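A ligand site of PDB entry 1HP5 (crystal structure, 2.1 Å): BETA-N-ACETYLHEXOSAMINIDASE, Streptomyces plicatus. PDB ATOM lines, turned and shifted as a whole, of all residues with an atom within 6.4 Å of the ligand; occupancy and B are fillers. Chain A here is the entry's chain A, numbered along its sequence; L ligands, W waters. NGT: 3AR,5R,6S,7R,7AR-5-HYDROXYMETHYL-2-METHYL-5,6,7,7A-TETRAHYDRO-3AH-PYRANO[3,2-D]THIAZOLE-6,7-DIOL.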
ATOM      1  N   ASP A 165      -5.527  23.143  -0.222  1.00  0.00           N
ATOM      2  CA  ASP A 165      -5.802  22.445   1.020  1.00  0.00           C
ATOM      3  C   ASP A 165      -7.273  22.022   0.982  1.00  0.00           C
ATOM      4  O   ASP A 165      -8.168  22.877   0.995  1.00  0.00           O
ATOM      5  CB  ASP A 165      -5.538  23.406   2.196  1.00  0.00           C
ATOM      6  CG  ASP A 165      -6.060  22.885   3.532  1.00  0.00           C
ATOM      7  OD1 ASP A 165      -6.530  21.724   3.606  1.00  0.00           O
ATOM      8  OD2 ASP A 165      -5.987  23.649   4.518  1.00  0.00           O
ATOM      9  N   ARG A 168      -8.881  21.284   5.490  1.00  0.00           N
ATOM     10  CA  ARG A 168      -9.529  22.241   6.388  1.00  0.00           C
ATOM     11  C   ARG A 168     -10.982  22.406   5.962  1.00  0.00           C
ATOM     12  O   ARG A 168     -11.898  22.314   6.782  1.00  0.00           O
ATOM     13  CB  ARG A 168      -8.780  23.572   6.379  1.00  0.00           C
ATOM     14  CG  ARG A 168      -7.561  23.566   7.303  1.00  0.00           C
ATOM     15  CD  ARG A 168      -6.828  22.209   7.345  1.00  0.00           C
ATOM     16  NE  ARG A 168      -5.758  22.237   8.339  1.00  0.00           N
ATOM     17  CZ  ARG A 168      -4.591  22.845   8.155  1.00  0.00           C
ATOM     18  NH1 ARG A 168      -4.334  23.464   7.010  1.00  0.00           N
ATOM     19  NH2 ARG A 168      -3.693  22.867   9.127  1.00  0.00           N
ATOM     20  N   HIS A 194      -3.254  18.839  -0.488  1.00  0.00           N
ATOM     21  CA  HIS A 194      -3.094  18.551   0.930  1.00  0.00           C
ATOM     22  C   HIS A 194      -4.333  17.719   1.277  1.00  0.00           C
ATOM     23  O   HIS A 194      -5.375  18.261   1.657  1.00  0.00           O
ATOM     24  CB  HIS A 194      -3.092  19.870   1.716  1.00  0.00           C
ATOM     25  CG  HIS A 194      -2.585  19.742   3.115  1.00  0.00           C
ATOM     26  ND1 HIS A 194      -1.238  19.642   3.413  1.00  0.00           N
ATOM     27  CD2 HIS A 194      -3.240  19.730   4.305  1.00  0.00           C
ATOM     28  CE1 HIS A 194      -1.085  19.551   4.724  1.00  0.00           C
ATOM     29  NE2 HIS A 194      -2.286  19.613   5.285  1.00  0.00           N
ATOM     30  N   ASP A 197      -5.224  16.249   7.198  1.00  0.00           N
ATOM     31  CA  ASP A 197      -4.755  17.125   8.243  1.00  0.00           C
ATOM     32  C   ASP A 197      -5.530  16.812   9.511  1.00  0.00           C
ATOM     33  O   ASP A 197      -6.089  15.715   9.641  1.00  0.00           O
ATOM     34  CB  ASP A 197      -4.936  18.589   7.831  1.00  0.00           C
ATOM     35  CG  ASP A 197      -3.900  19.505   8.470  1.00  0.00           C
ATOM     36  OD1 ASP A 197      -4.053  19.829   9.664  1.00  0.00           O
ATOM     37  OD2 ASP A 197      -2.920  19.872   7.789  1.00  0.00           O
ATOM     38  N   ASP A 252       0.123  14.331   5.259  1.00  0.00           N
ATOM     39  CA  ASP A 252       0.968  14.929   6.291  1.00  0.00           C
ATOM     40  C   ASP A 252       1.249  13.999   7.467  1.00  0.00           C
ATOM     41  O   ASP A 252       0.322  13.400   8.022  1.00  0.00           O
ATOM     42  CB  ASP A 252       0.325  16.224   6.816  1.00  0.00           C
ATOM     43  CG  ASP A 252       1.344  17.233   7.301  1.00  0.00           C
ATOM     44  OD1 ASP A 252       2.446  16.821   7.729  1.00  0.00           O
ATOM     45  OD2 ASP A 252       1.051  18.451   7.273  1.00  0.00           O
ATOM     46  N   HIS A 256      -0.113  16.962  12.188  1.00  0.00           N
ATOM     47  CA  HIS A 256      -1.317  17.254  11.411  1.00  0.00           C
ATOM     48  C   HIS A 256      -2.020  15.942  11.025  1.00  0.00           C
ATOM     49  O   HIS A 256      -2.507  15.785   9.901  1.00  0.00           O
ATOM     50  CB  HIS A 256      -0.940  18.029  10.142  1.00  0.00           C
ATOM     51  CG  HIS A 256      -0.633  19.471  10.384  1.00  0.00           C
ATOM     52  ND1 HIS A 256      -1.619  20.425  10.528  1.00  0.00           N
ATOM     53  CD2 HIS A 256       0.540  20.116  10.564  1.00  0.00           C
ATOM     54  CE1 HIS A 256      -1.059  21.595  10.769  1.00  0.00           C
ATOM     55  NE2 HIS A 256       0.251  21.432  10.802  1.00  0.00           N
ATOM     56  N   VAL A 282      -2.994  24.479  15.185  1.00  0.00           N
ATOM     57  CA  VAL A 282      -2.119  23.395  14.727  1.00  0.00           C
ATOM     58  C   VAL A 282      -1.124  22.943  15.794  1.00  0.00           C
ATOM     59  O   VAL A 282      -1.021  23.567  16.853  1.00  0.00           O
ATOM     60  CB  VAL A 282      -1.278  23.854  13.509  1.00  0.00           C
ATOM     61  CG1 VAL A 282      -2.160  24.537  12.479  1.00  0.00           C
ATOM     62  CG2 VAL A 282      -0.177  24.819  13.967  1.00  0.00           C
ATOM     63  N   ASP A 319       5.491  19.009   8.725  1.00  0.00           N
ATOM     64  CA  ASP A 319       5.438  20.318   9.340  1.00  0.00           C
ATOM     65  C   ASP A 319       4.749  20.316  10.688  1.00  0.00           C
ATOM     66  O   ASP A 319       3.856  19.498  10.951  1.00  0.00           O
ATOM     67  CB  ASP A 319       4.683  21.299   8.423  1.00  0.00           C
ATOM     68  CG  ASP A 319       3.235  20.877   8.217  1.00  0.00           C
ATOM     69  OD1 ASP A 319       3.008  19.714   7.823  1.00  0.00           O
ATOM     70  OD2 ASP A 319       2.313  21.707   8.449  1.00  0.00           O
ATOM     71  N   GLU A 320       5.176  21.229  11.545  1.00  0.00           N
ATOM     72  CA  GLU A 320       4.579  21.425  12.861  1.00  0.00           C
ATOM     73  C   GLU A 320       4.242  20.174  13.662  1.00  0.00           C
ATOM     74  O   GLU A 320       3.136  20.056  14.201  1.00  0.00           O
ATOM     75  CB  GLU A 320       3.322  22.282  12.699  1.00  0.00           C
ATOM     76  CG  GLU A 320       3.553  23.466  11.775  1.00  0.00           C
ATOM     77  CD  GLU A 320       2.316  24.321  11.588  1.00  0.00           C
ATOM     78  OE1 GLU A 320       1.239  23.775  11.249  1.00  0.00           O
ATOM     79  OE2 GLU A 320       2.428  25.555  11.762  1.00  0.00           O
ATOM     80  N   TRP A 350       7.924  19.149   3.956  1.00  0.00           N
ATOM     81  CA  TRP A 350       8.071  20.556   4.298  1.00  0.00           C
ATOM     82  C   TRP A 350       9.509  20.664   4.797  1.00  0.00           C
ATOM     83  O   TRP A 350      10.113  19.634   5.131  1.00  0.00           O
ATOM     84  CB  TRP A 350       7.050  20.959   5.346  1.00  0.00           C
ATOM     85  CG  TRP A 350       5.646  20.875   4.817  1.00  0.00           C
ATOM     86  CD1 TRP A 350       4.719  19.910   5.086  1.00  0.00           C
ATOM     87  CD2 TRP A 350       5.024  21.781   3.893  1.00  0.00           C
ATOM     88  NE1 TRP A 350       3.553  20.166   4.394  1.00  0.00           N
ATOM     89  CE2 TRP A 350       3.719  21.300   3.651  1.00  0.00           C
ATOM     90  CE3 TRP A 350       5.455  22.950   3.249  1.00  0.00           C
ATOM     91  CZ2 TRP A 350       2.827  21.948   2.794  1.00  0.00           C
ATOM     92  CZ3 TRP A 350       4.563  23.598   2.393  1.00  0.00           C
ATOM     93  CH2 TRP A 350       3.268  23.098   2.173  1.00  0.00           C
ATOM     94  N   GLN A 352      10.950  21.092   7.488  1.00  0.00           N
ATOM     95  CA  GLN A 352      11.334  20.528   8.784  1.00  0.00           C
ATOM     96  C   GLN A 352      12.064  19.214   8.509  1.00  0.00           C
ATOM     97  O   GLN A 352      12.838  18.748   9.344  1.00  0.00           O
ATOM     98  CB  GLN A 352      10.105  20.234   9.667  1.00  0.00           C
ATOM     99  CG  GLN A 352       9.512  21.442  10.357  1.00  0.00           C
ATOM    100  CD  GLN A 352       9.014  22.482   9.389  1.00  0.00           C
ATOM    101  OE1 GLN A 352       8.351  22.155   8.398  1.00  0.00           O
ATOM    102  NE2 GLN A 352       9.329  23.743   9.647  1.00  0.00           N
ATOM    103  N   TRP A 367       8.785  26.865   3.850  1.00  0.00           N
ATOM    104  CA  TRP A 367       7.647  27.735   4.087  1.00  0.00           C
ATOM    105  C   TRP A 367       7.919  28.795   5.142  1.00  0.00           C
ATOM    106  O   TRP A 367       6.981  29.329   5.749  1.00  0.00           O
ATOM    107  CB  TRP A 367       6.407  26.916   4.486  1.00  0.00           C
ATOM    108  CG  TRP A 367       6.586  26.040   5.684  1.00  0.00           C
ATOM    109  CD1 TRP A 367       7.267  24.860   5.753  1.00  0.00           C
ATOM    110  CD2 TRP A 367       6.041  26.265   6.993  1.00  0.00           C
ATOM    111  NE1 TRP A 367       7.182  24.333   7.012  1.00  0.00           N
ATOM    112  CE2 TRP A 367       6.436  25.174   7.798  1.00  0.00           C
ATOM    113  CE3 TRP A 367       5.261  27.276   7.562  1.00  0.00           C
ATOM    114  CZ2 TRP A 367       6.077  25.065   9.148  1.00  0.00           C
ATOM    115  CZ3 TRP A 367       4.902  27.167   8.912  1.00  0.00           C
ATOM    116  CH2 TRP A 367       5.314  26.067   9.687  1.00  0.00           C
ATOM    117  N   ALA A 395       5.993  31.877   3.469  1.00  0.00           N
ATOM    118  CA  ALA A 395       4.690  32.227   4.014  1.00  0.00           C
ATOM    119  C   ALA A 395       4.359  33.714   3.863  1.00  0.00           C
ATOM    120  O   ALA A 395       3.188  34.088   3.779  1.00  0.00           O
ATOM    121  CB  ALA A 395       4.623  31.831   5.487  1.00  0.00           C
ATOM    122  N   TYR A 399       1.948  32.447   0.050  1.00  0.00           N
ATOM    123  CA  TYR A 399       0.779  31.859   0.697  1.00  0.00           C
ATOM    124  C   TYR A 399      -0.446  32.663   0.278  1.00  0.00           C
ATOM    125  O   TYR A 399      -0.614  33.808   0.677  1.00  0.00           O
ATOM    126  CB  TYR A 399       0.953  31.886   2.221  1.00  0.00           C
ATOM    127  CG  TYR A 399       1.663  30.653   2.768  1.00  0.00           C
ATOM    128  CD1 TYR A 399       2.701  30.051   2.053  1.00  0.00           C
ATOM    129  CD2 TYR A 399       1.272  30.072   3.971  1.00  0.00           C
ATOM    130  CE1 TYR A 399       3.314  28.904   2.507  1.00  0.00           C
ATOM    131  CE2 TYR A 399       1.891  28.920   4.447  1.00  0.00           C
ATOM    132  CZ  TYR A 399       2.904  28.334   3.704  1.00  0.00           C
ATOM    133  OH  TYR A 399       3.490  27.152   4.113  1.00  0.00           O
ATOM    134  N   ASP A 401      -3.391  32.232   1.206  1.00  0.00           N
ATOM    135  CA  ASP A 401      -4.349  32.387   2.301  1.00  0.00           C
ATOM    136  C   ASP A 401      -3.978  33.562   3.191  1.00  0.00           C
ATOM    137  O   ASP A 401      -4.731  33.926   4.071  1.00  0.00           O
ATOM    138  CB  ASP A 401      -4.441  31.108   3.137  1.00  0.00           C
ATOM    139  CG  ASP A 401      -3.141  30.777   3.840  1.00  0.00           C
ATOM    140  OD1 ASP A 401      -2.083  30.776   3.170  1.00  0.00           O
ATOM    141  OD2 ASP A 401      -3.170  30.505   5.059  1.00  0.00           O
ATOM    142  N   MET A 402      -2.807  34.164   2.961  1.00  0.00           N
ATOM    143  CA  MET A 402      -2.392  35.293   3.808  1.00  0.00           C
ATOM    144  C   MET A 402      -3.115  36.565   3.372  1.00  0.00           C
ATOM    145  O   MET A 402      -3.246  36.840   2.184  1.00  0.00           O
ATOM    146  CB  MET A 402      -0.877  35.504   3.732  1.00  0.00           C
ATOM    147  CG  MET A 402      -0.244  35.934   5.049  1.00  0.00           C
ATOM    148  SD  MET A 402      -0.571  34.733   6.370  1.00  0.00           S
ATOM    149  CE  MET A 402       0.232  33.256   5.675  1.00  0.00           C
ATOM    150  N   LEU A 412      -5.396  34.487   6.752  1.00  0.00           N
ATOM    151  CA  LEU A 412      -4.689  34.564   8.011  1.00  0.00           C
ATOM    152  C   LEU A 412      -3.674  35.700   7.960  1.00  0.00           C
ATOM    153  O   LEU A 412      -3.501  36.339   6.929  1.00  0.00           O
ATOM    154  CB  LEU A 412      -3.972  33.243   8.309  1.00  0.00           C
ATOM    155  CG  LEU A 412      -4.912  32.030   8.397  1.00  0.00           C
ATOM    156  CD1 LEU A 412      -4.096  30.770   8.708  1.00  0.00           C
ATOM    157  CD2 LEU A 412      -5.953  32.282   9.485  1.00  0.00           C
ATOM    158  N   TRP A 414      -0.683  35.420  10.363  1.00  0.00           N
ATOM    159  CA  TRP A 414       0.421  35.021  11.225  1.00  0.00           C
ATOM    160  C   TRP A 414       1.760  35.353  10.574  1.00  0.00           C
ATOM    161  O   TRP A 414       2.739  35.597  11.279  1.00  0.00           O
ATOM    162  CB  TRP A 414       0.348  33.532  11.555  1.00  0.00           C
ATOM    163  CG  TRP A 414       0.514  32.605  10.390  1.00  0.00           C
ATOM    164  CD1 TRP A 414      -0.473  32.091   9.602  1.00  0.00           C
ATOM    165  CD2 TRP A 414       1.751  32.070   9.897  1.00  0.00           C
ATOM    166  NE1 TRP A 414       0.076  31.255   8.651  1.00  0.00           N
ATOM    167  CE2 TRP A 414       1.437  31.227   8.811  1.00  0.00           C
ATOM    168  CE3 TRP A 414       3.086  32.220  10.279  1.00  0.00           C
ATOM    169  CZ2 TRP A 414       2.419  30.531   8.091  1.00  0.00           C
ATOM    170  CZ3 TRP A 414       4.068  31.524   9.560  1.00  0.00           C
ATOM    171  CH2 TRP A 414       3.719  30.686   8.481  1.00  0.00           C
ATOM    172  N   TRP A 448      -4.113  27.553   1.709  1.00  0.00           N
ATOM    173  CA  TRP A 448      -4.660  26.847   2.871  1.00  0.00           C
ATOM    174  C   TRP A 448      -6.113  27.298   3.049  1.00  0.00           C
ATOM    175  O   TRP A 448      -6.444  28.445   2.767  1.00  0.00           O
ATOM    176  CB  TRP A 448      -3.845  27.148   4.127  1.00  0.00           C
ATOM    177  CG  TRP A 448      -2.407  26.774   3.957  1.00  0.00           C
ATOM    178  CD1 TRP A 448      -1.383  27.604   3.584  1.00  0.00           C
ATOM    179  CD2 TRP A 448      -1.840  25.469   4.088  1.00  0.00           C
ATOM    180  NE1 TRP A 448      -0.210  26.886   3.475  1.00  0.00           N
ATOM    181  CE2 TRP A 448      -0.468  25.576   3.780  1.00  0.00           C
ATOM    182  CE3 TRP A 448      -2.367  24.216   4.435  1.00  0.00           C
ATOM    183  CZ2 TRP A 448       0.394  24.471   3.808  1.00  0.00           C
ATOM    184  CZ3 TRP A 448      -1.505  23.111   4.462  1.00  0.00           C
ATOM    185  CH2 TRP A 448      -0.138  23.253   4.144  1.00  0.00           C
ATOM    186  N   THR A 449      -6.954  26.415   3.551  1.00  0.00           N
ATOM    187  CA  THR A 449      -8.366  26.761   3.662  1.00  0.00           C
ATOM    188  C   THR A 449      -9.038  26.844   5.027  1.00  0.00           C
ATOM    189  O   THR A 449     -10.236  26.602   5.147  1.00  0.00           O
ATOM    190  CB  THR A 449      -9.187  25.817   2.759  1.00  0.00           C
ATOM    191  OG1 THR A 449      -8.947  24.463   3.135  1.00  0.00           O
ATOM    192  CG2 THR A 449      -8.762  25.996   1.286  1.00  0.00           C
ATOM    193  N   GLU A 450      -8.274  27.210   6.061  1.00  0.00           N
ATOM    194  CA  GLU A 450      -8.878  27.354   7.383  1.00  0.00           C
ATOM    195  C   GLU A 450     -10.074  28.304   7.311  1.00  0.00           C
ATOM    196  O   GLU A 450     -11.087  28.083   7.966  1.00  0.00           O
ATOM    197  CB  GLU A 450      -7.887  27.923   8.408  1.00  0.00           C
ATOM    198  CG  GLU A 450      -6.955  26.910   9.046  1.00  0.00           C
ATOM    199  CD  GLU A 450      -5.634  26.780   8.317  1.00  0.00           C
ATOM    200  OE1 GLU A 450      -5.585  27.072   7.098  1.00  0.00           O
ATOM    201  OE2 GLU A 450      -4.647  26.371   8.963  1.00  0.00           O
HETATM  202  C1  NGT L   1       1.350  26.548   8.079  1.00  0.00           C
HETATM  203  C2  NGT L   1       0.853  25.133   8.492  1.00  0.00           C
HETATM  204  C3  NGT L   1      -0.568  24.820   7.898  1.00  0.00           C
HETATM  205  C4  NGT L   1      -1.522  26.024   7.986  1.00  0.00           C
HETATM  206  C5  NGT L   1      -0.878  27.269   7.339  1.00  0.00           C
HETATM  207  C6  NGT L   1      -1.747  28.516   7.400  1.00  0.00           C
HETATM  208  C7  NGT L   1       2.468  24.567   6.972  1.00  0.00           C
HETATM  209  C8  NGT L   1       3.491  23.766   6.203  1.00  0.00           C
HETATM  210  N2  NGT L   1       1.815  24.159   7.967  1.00  0.00           N
HETATM  211  S1  NGT L   1       2.167  26.223   6.439  1.00  0.00           S
HETATM  212  O3  NGT L   1      -1.119  23.694   8.554  1.00  0.00           O
HETATM  213  O4  NGT L   1      -2.728  25.701   7.313  1.00  0.00           O
HETATM  214  O5  NGT L   1       0.406  27.582   8.008  1.00  0.00           O
HETATM  215  O6  NGT L   1      -1.168  29.579   6.644  1.00  0.00           O
HETATM  216  O   HOH W   1      -0.389  21.396   7.542  1.00  0.00           O
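OE1 of Glu 320 lies close to N2 of the ligand (3.4 Å). Merely in contact with the ligand: Trp 350, Trp 367, Leu 412 and Trp 448. Hydrophobic or aromatic side chains within 4 Å of the ligand: His 256, Trp 350, Trp 367, Tyr 399, Leu 412, Trp 414 and Trp 448. Within 4 Å of the ligand: Arg 168, His 256, Asp 319, Glu 320, Trp 350, Trp 367, Tyr 399, Asp 401, Leu 412, Trp 414, Trp 448 and Glu 450.
The side-chain carboxylate of Asp 319 is in hydrogen-bond range of a ring nitrogen (NE2) of His 256. NH2 of Arg 168 lies within salt-bridge range of OD1 of Asp 197 (3.1 Å). The guanidinium group of Arg 168 lies within salt-bridge range of the side-chain carboxylate of Asp 165, 3.0 Å away. NH2 of Arg 168 sits close to ND1 of His 256, 3.5 Å away. The side-chain amide oxygen (OE1) of Gln 352 sits at hydrogen-bond distance from the indole nitrogen (NE1) of Trp 367. NE2 of His 256 sits at hydrogen-bond distance from OE1 of Glu 320. ND1 of His 256 sits at hydrogen-bond distance from OD1 of Asp 197, at 2.7 Å. OE2 of Glu 450 lies within salt-bridge range of NH1 of Arg 168.
The side-chain carboxylate (OE2) of Glu 450 lies within hydrogen-bond range of an oxygen (O4) of the ligand, 2.6 Å away. The side-chain carboxylate (OD2) of Asp 401 lies within hydrogen-bond range of an oxygen (O6) of the ligand. The side-chain carboxylate (OD2) of Asp 319 lies within hydrogen-bond range of a nitrogen (N2) of the ligand (2.5 Å). O6 of the ligand is in hydrogen-bond range of NE1 of Trp 414. A ring nitrogen (NE2) of His 256 lies close to an oxygen (O3) of the ligand. A sulfur (S1) of the ligand lies close to the side-chain hydroxyl (OH) of Tyr 399 (2.8 Å). O3 of the ligand lies within hydrogen-bond range of NH2 of Arg 168 (2.8 Å).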
